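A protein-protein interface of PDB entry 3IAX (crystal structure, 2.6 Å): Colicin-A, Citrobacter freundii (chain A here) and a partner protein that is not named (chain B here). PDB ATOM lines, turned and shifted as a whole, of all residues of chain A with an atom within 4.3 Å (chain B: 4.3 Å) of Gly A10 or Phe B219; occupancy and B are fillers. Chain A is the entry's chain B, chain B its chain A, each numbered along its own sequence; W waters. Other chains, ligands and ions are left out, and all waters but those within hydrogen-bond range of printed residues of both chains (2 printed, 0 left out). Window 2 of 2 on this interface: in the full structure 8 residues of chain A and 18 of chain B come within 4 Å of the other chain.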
ATOM      1  N   LYS A   9      19.969 -31.253  26.106  1.00  0.00           N
ATOM      2  CA  LYS A   9      19.998 -29.806  25.707  1.00  0.00           C
ATOM      3  C   LYS A   9      18.607 -29.251  25.379  1.00  0.00           C
ATOM      4  O   LYS A   9      18.107 -29.399  24.266  1.00  0.00           O
ATOM      5  CB  LYS A   9      20.971 -29.573  24.537  1.00  0.00           C
ATOM      6  CG  LYS A   9      22.154 -28.663  24.890  1.00  0.00           C
ATOM      7  CD  LYS A   9      23.214 -29.352  25.750  1.00  0.00           C
ATOM      8  CE  LYS A   9      24.350 -29.873  24.856  1.00  0.00           C
ATOM      9  NZ  LYS A   9      24.881 -31.183  25.471  1.00  0.00           N
ATOM     10  N   GLY A  10      17.990 -28.596  26.363  1.00  0.00           N
ATOM     11  CA  GLY A  10      16.594 -28.155  26.237  1.00  0.00           C
ATOM     12  C   GLY A  10      16.061 -27.665  27.566  1.00  0.00           C
ATOM     13  O   GLY A  10      16.803 -27.601  28.556  1.00  0.00           O
ATOM     14  N   ASP A  11      14.780 -27.298  27.595  1.00  0.00           N
ATOM     15  CA  ASP A  11      14.211 -26.762  28.826  1.00  0.00           C
ATOM     16  C   ASP A  11      13.441 -27.813  29.630  1.00  0.00           C
ATOM     17  O   ASP A  11      13.007 -27.543  30.749  1.00  0.00           O
ATOM     18  CB  ASP A  11      13.390 -25.475  28.573  1.00  0.00           C
ATOM     19  CG  ASP A  11      12.028 -25.735  27.926  1.00  0.00           C
ATOM     20  OD1 ASP A  11      11.673 -26.905  27.640  1.00  0.00           O
ATOM     21  OD2 ASP A  11      11.298 -24.746  27.701  1.00  0.00           O
ATOM     22  N   GLY A  12      13.291 -29.003  29.048  1.00  0.00           N
ATOM     23  CA  GLY A  12      12.609 -30.122  29.698  1.00  0.00           C
ATOM     24  C   GLY A  12      11.134 -29.869  29.948  1.00  0.00           C
ATOM     25  O   GLY A  12      10.640 -30.074  31.060  1.00  0.00           O
ATOM     26  N   GLU A  18      11.531 -24.324  23.178  1.00  0.00           N
ATOM     27  CA  GLU A  18      12.859 -24.572  23.639  1.00  0.00           C
ATOM     28  C   GLU A  18      13.102 -25.905  24.291  1.00  0.00           C
ATOM     29  O   GLU A  18      13.817 -25.965  25.231  1.00  0.00           O
ATOM     30  CB  GLU A  18      13.199 -23.499  24.640  1.00  0.00           C
ATOM     31  CG  GLU A  18      13.431 -22.193  24.055  1.00  0.00           C
ATOM     32  CD  GLU A  18      13.878 -21.195  25.033  1.00  0.00           C
ATOM     33  OE1 GLU A  18      13.734 -21.385  26.197  1.00  0.00           O
ATOM     34  OE2 GLU A  18      14.360 -20.177  24.635  1.00  0.00           O
ATOM     35  N   ARG A  19      12.530 -26.976  23.783  1.00  0.00           N
ATOM     36  CA  ARG A  19      12.641 -28.320  24.383  1.00  0.00           C
ATOM     37  C   ARG A  19      13.878 -29.074  23.960  1.00  0.00           C
ATOM     38  O   ARG A  19      14.496 -29.744  24.781  1.00  0.00           O
ATOM     39  CB  ARG A  19      11.471 -29.224  24.006  1.00  0.00           C
ATOM     40  CG  ARG A  19      10.287 -28.574  23.396  1.00  0.00           C
ATOM     41  CD  ARG A  19       9.657 -29.543  22.415  1.00  0.00           C
ATOM     42  NE  ARG A  19       9.799 -29.074  21.043  1.00  0.00           N
ATOM     43  CZ  ARG A  19       8.795 -28.972  20.177  1.00  0.00           C
ATOM     44  NH1 ARG A  19       7.563 -29.337  20.535  1.00  0.00           N
ATOM     45  NH2 ARG A  19       9.023 -28.526  18.948  1.00  0.00           N
ATOM     46  N   GLN B 200      27.596 -25.564  20.125  1.00  0.00           N
ATOM     47  CA  GLN B 200      26.318 -25.931  20.671  1.00  0.00           C
ATOM     48  C   GLN B 200      25.138 -25.165  20.157  1.00  0.00           C
ATOM     49  O   GLN B 200      25.264 -24.331  19.346  1.00  0.00           O
ATOM     50  CB  GLN B 200      26.361 -25.907  22.175  1.00  0.00           C
ATOM     51  CG  GLN B 200      27.570 -26.523  22.724  1.00  0.00           C
ATOM     52  CD  GLN B 200      27.607 -28.013  22.601  1.00  0.00           C
ATOM     53  OE1 GLN B 200      26.602 -28.650  22.556  1.00  0.00           O
ATOM     54  NE2 GLN B 200      28.780 -28.558  22.544  1.00  0.00           N
ATOM     55  N   PRO B 201      23.973 -25.470  20.647  1.00  0.00           N
ATOM     56  CA  PRO B 201      22.789 -24.829  20.165  1.00  0.00           C
ATOM     57  C   PRO B 201      22.535 -23.449  20.700  1.00  0.00           C
ATOM     58  O   PRO B 201      22.853 -23.113  21.786  1.00  0.00           O
ATOM     59  CB  PRO B 201      21.709 -25.806  20.567  1.00  0.00           C
ATOM     60  CG  PRO B 201      22.298 -26.952  20.659  1.00  0.00           C
ATOM     61  CD  PRO B 201      23.634 -26.780  21.148  1.00  0.00           C
ATOM     62  N   MET B 203      19.348 -20.612  20.973  1.00  0.00           N
ATOM     63  CA  MET B 203      17.917 -20.465  20.908  1.00  0.00           C
ATOM     64  C   MET B 203      17.470 -19.076  21.116  1.00  0.00           C
ATOM     65  O   MET B 203      18.141 -18.281  21.698  1.00  0.00           O
ATOM     66  CB  MET B 203      17.259 -21.298  21.957  1.00  0.00           C
ATOM     67  CG  MET B 203      17.770 -22.658  22.078  1.00  0.00           C
ATOM     68  SD  MET B 203      16.835 -23.568  23.220  1.00  0.00           S
ATOM     69  CE  MET B 203      16.389 -24.801  22.201  1.00  0.00           C
ATOM     70  N   VAL B 217      19.813 -17.448  23.942  1.00  0.00           N
ATOM     71  CA  VAL B 217      20.250 -18.561  24.776  1.00  0.00           C
ATOM     72  C   VAL B 217      21.363 -19.262  24.039  1.00  0.00           C
ATOM     73  O   VAL B 217      21.241 -19.525  22.845  1.00  0.00           O
ATOM     74  CB  VAL B 217      19.115 -19.566  24.984  1.00  0.00           C
ATOM     75  CG1 VAL B 217      19.547 -20.689  25.917  1.00  0.00           C
ATOM     76  CG2 VAL B 217      17.877 -18.852  25.514  1.00  0.00           C
ATOM     77  N   THR B 218      22.449 -19.547  24.733  1.00  0.00           N
ATOM     78  CA  THR B 218      23.540 -20.330  24.170  1.00  0.00           C
ATOM     79  C   THR B 218      23.862 -21.500  25.077  1.00  0.00           C
ATOM     80  O   THR B 218      23.723 -21.391  26.291  1.00  0.00           O
ATOM     81  CB  THR B 218      24.826 -19.485  23.959  1.00  0.00           C
ATOM     82  OG1 THR B 218      25.872 -20.345  23.492  1.00  0.00           O
ATOM     83  CG2 THR B 218      25.281 -18.779  25.243  1.00  0.00           C
ATOM     84  N   PHE B 219      24.287 -22.615  24.489  1.00  0.00           N
ATOM     85  CA  PHE B 219      24.705 -23.786  25.260  1.00  0.00           C
ATOM     86  C   PHE B 219      26.209 -24.023  25.159  1.00  0.00           C
ATOM     87  O   PHE B 219      26.721 -25.034  25.649  1.00  0.00           O
ATOM     88  CB  PHE B 219      23.932 -25.024  24.813  1.00  0.00           C
ATOM     89  CG  PHE B 219      22.487 -25.026  25.233  1.00  0.00           C
ATOM     90  CD1 PHE B 219      21.531 -24.318  24.497  1.00  0.00           C
ATOM     91  CD2 PHE B 219      22.076 -25.749  26.365  1.00  0.00           C
ATOM     92  CE1 PHE B 219      20.182 -24.323  24.873  1.00  0.00           C
ATOM     93  CE2 PHE B 219      20.733 -25.768  26.768  1.00  0.00           C
ATOM     94  CZ  PHE B 219      19.778 -25.048  26.024  1.00  0.00           C
ATOM     95  N   GLU B 220      26.902 -23.063  24.616  1.00  0.00           N
ATOM     96  CA  GLU B 220      28.322 -23.070  24.462  1.00  0.00           C
ATOM     97  C   GLU B 220      29.121 -23.617  25.634  1.00  0.00           C
ATOM     98  O   GLU B 220      30.128 -24.214  25.451  1.00  0.00           O
ATOM     99  CB  GLU B 220      28.760 -21.664  24.138  1.00  0.00           C
ATOM    100  CG  GLU B 220      29.284 -21.507  22.799  1.00  0.00           C
ATOM    101  CD  GLU B 220      29.108 -20.142  22.202  1.00  0.00           C
ATOM    102  OE1 GLU B 220      29.985 -19.721  21.475  1.00  0.00           O
ATOM    103  OE2 GLU B 220      28.109 -19.485  22.420  1.00  0.00           O
ATOM    104  N   SER B 221      28.654 -23.402  26.839  1.00  0.00           N
ATOM    105  CA  SER B 221      29.331 -23.847  28.031  1.00  0.00           C
ATOM    106  C   SER B 221      29.184 -25.316  28.421  1.00  0.00           C
ATOM    107  O   SER B 221      29.966 -25.821  29.157  1.00  0.00           O
ATOM    108  CB  SER B 221      28.908 -22.983  29.196  1.00  0.00           C
ATOM    109  OG  SER B 221      27.529 -22.805  29.251  1.00  0.00           O
ATOM    110  N   GLY B 222      28.156 -25.960  27.925  1.00  0.00           N
ATOM    111  CA  GLY B 222      27.834 -27.314  28.222  1.00  0.00           C
ATOM    112  C   GLY B 222      26.464 -27.177  28.778  1.00  0.00           C
ATOM    113  O   GLY B 222      25.663 -28.070  28.769  1.00  0.00           O
ATOM    114  N   ARG B 223      26.219 -25.985  29.252  1.00  0.00           N
ATOM    115  CA  ARG B 223      25.028 -25.606  29.935  1.00  0.00           C
ATOM    116  C   ARG B 223      24.358 -24.416  29.268  1.00  0.00           C
ATOM    117  O   ARG B 223      24.985 -23.677  28.572  1.00  0.00           O
ATOM    118  CB  ARG B 223      25.530 -25.163  31.294  1.00  0.00           C
ATOM    119  CG  ARG B 223      24.657 -25.413  32.427  1.00  0.00           C
ATOM    120  CD  ARG B 223      25.390 -25.518  33.732  1.00  0.00           C
ATOM    121  NE  ARG B 223      26.067 -24.345  34.276  1.00  0.00           N
ATOM    122  CZ  ARG B 223      25.477 -23.247  34.672  1.00  0.00           C
ATOM    123  NH1 ARG B 223      24.193 -23.109  34.531  1.00  0.00           N
ATOM    124  NH2 ARG B 223      26.177 -22.296  35.200  1.00  0.00           N
ATOM    125  N   SER B 224      23.059 -24.260  29.508  1.00  0.00           N
ATOM    126  CA  SER B 224      22.302 -23.157  28.931  1.00  0.00           C
ATOM    127  C   SER B 224      22.639 -21.838  29.620  1.00  0.00           C
ATOM    128  O   SER B 224      22.806 -21.788  30.839  1.00  0.00           O
ATOM    129  CB  SER B 224      20.800 -23.430  29.027  1.00  0.00           C
ATOM    130  OG  SER B 224      20.261 -22.909  30.230  1.00  0.00           O
ATOM    131  N   HIS B 245      17.917 -24.184  33.879  1.00  0.00           N
ATOM    132  CA  HIS B 245      17.563 -23.650  32.569  1.00  0.00           C
ATOM    133  C   HIS B 245      17.584 -22.125  32.572  1.00  0.00           C
ATOM    134  O   HIS B 245      17.285 -21.492  33.584  1.00  0.00           O
ATOM    135  CB  HIS B 245      16.185 -24.156  32.137  1.00  0.00           C
ATOM    136  CG  HIS B 245      15.860 -23.874  30.703  1.00  0.00           C
ATOM    137  ND1 HIS B 245      16.630 -24.341  29.660  1.00  0.00           N
ATOM    138  CD2 HIS B 245      14.848 -23.173  30.140  1.00  0.00           C
ATOM    139  CE1 HIS B 245      16.106 -23.939  28.515  1.00  0.00           C
ATOM    140  NE2 HIS B 245      15.025 -23.228  28.779  1.00  0.00           N
HETATM  141  O   HOH W   1      18.516 -26.250  29.901  1.00  0.00           O
HETATM  142  O   HOH W   2      11.832 -22.291  28.257  1.00  0.00           O
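OE1 of Glu A18 lies within hydrogen-bond range of NE2 of His B245 (3.4 Å). A ring nitrogen (ND1) of His B245 is in hydrogen-bond range of the backbone carbonyl oxygen (O) of Gly A10 (3.4 Å).
N of Phe B219 sits at hydrogen-bond distance from O of Pro B201, at 3.1 Å. The backbone NH of Asp A11 is in hydrogen-bond range of the backbone carbonyl oxygen of Glu A18 (2.9 Å). O of Val B217 lies within hydrogen-bond range of N of Met B203 (2.9 Å).
Gln B200 touches Lys A9 (OE1 to CE, 3.4 Å). CG of Lys A9 touches CD2 of Phe B219 (3.3 Å). Gly A10 touches Phe B219. NE2 of His B245 touches CB of Asp A11 (2.8 Å). Glu A18 touches Met B203 (CG to SD, 3.8 Å). CG2 of Val B217 touches OE2 of Glu A18, at 3.9 Å.
Gly A10 touches just these residues of chain B: Phe B219 and His B245. Phe B219 touches just these residues of chain A: Lys A9 (3.3 Å) and Gly A10 (3.96 Å). Of the printed residues of chain B, Asp A11 touches His B245 (2.8 Å). Printed residues of chain B within 4 Å of Lys A9: Gln B200 and Phe B219. Of the printed residues of chain A, Gln B200 touches Lys A9. Printed residues of chain B within 4 Å of Glu A18: Met B203, Val B217 and His B245. Of the printed residues of chain A, His B245 touches Gly A10 (3.4 Å), Asp A11 (2.8 Å) and Glu A18 (3.4 Å). Glu B220 touches none of the printed residues of chain A. Arg A19 touches none of the printed residues of chain B. The nearest printed residue of chain B that does not touch Gly A10 is Met B203 (5.3 Å). The nearest printed residue of chain B that does not touch Lys A9 is Gly B222 (4.1 Å).
Of the 6 printed residues of chain A, 4 touch a printed residue of chain B. Printed residues of chain A that touch a printed residue of chain B: Lys A9, Gly A10, Asp A11 and Glu A18. Of the 12 printed residues of chain B, 5 touch a printed residue of chain A. Printed residues of chain B that touch a printed residue of chain A: Gln B200, Met B203, Val B217, Phe B219 and His B245.
Water W1 lies within hydrogen-bond range of the backbone carbonyl oxygen (O) of Gly A10 (2.6 Å) and a ring nitrogen (ND1) of His B245 (2.7 Å). Water W2 lies within hydrogen-bond range of OD2 of Asp A11 (2.6 Å), OE1 of Glu A18 (2.9 Å) and NE2 of His B245 (3.4 Å).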
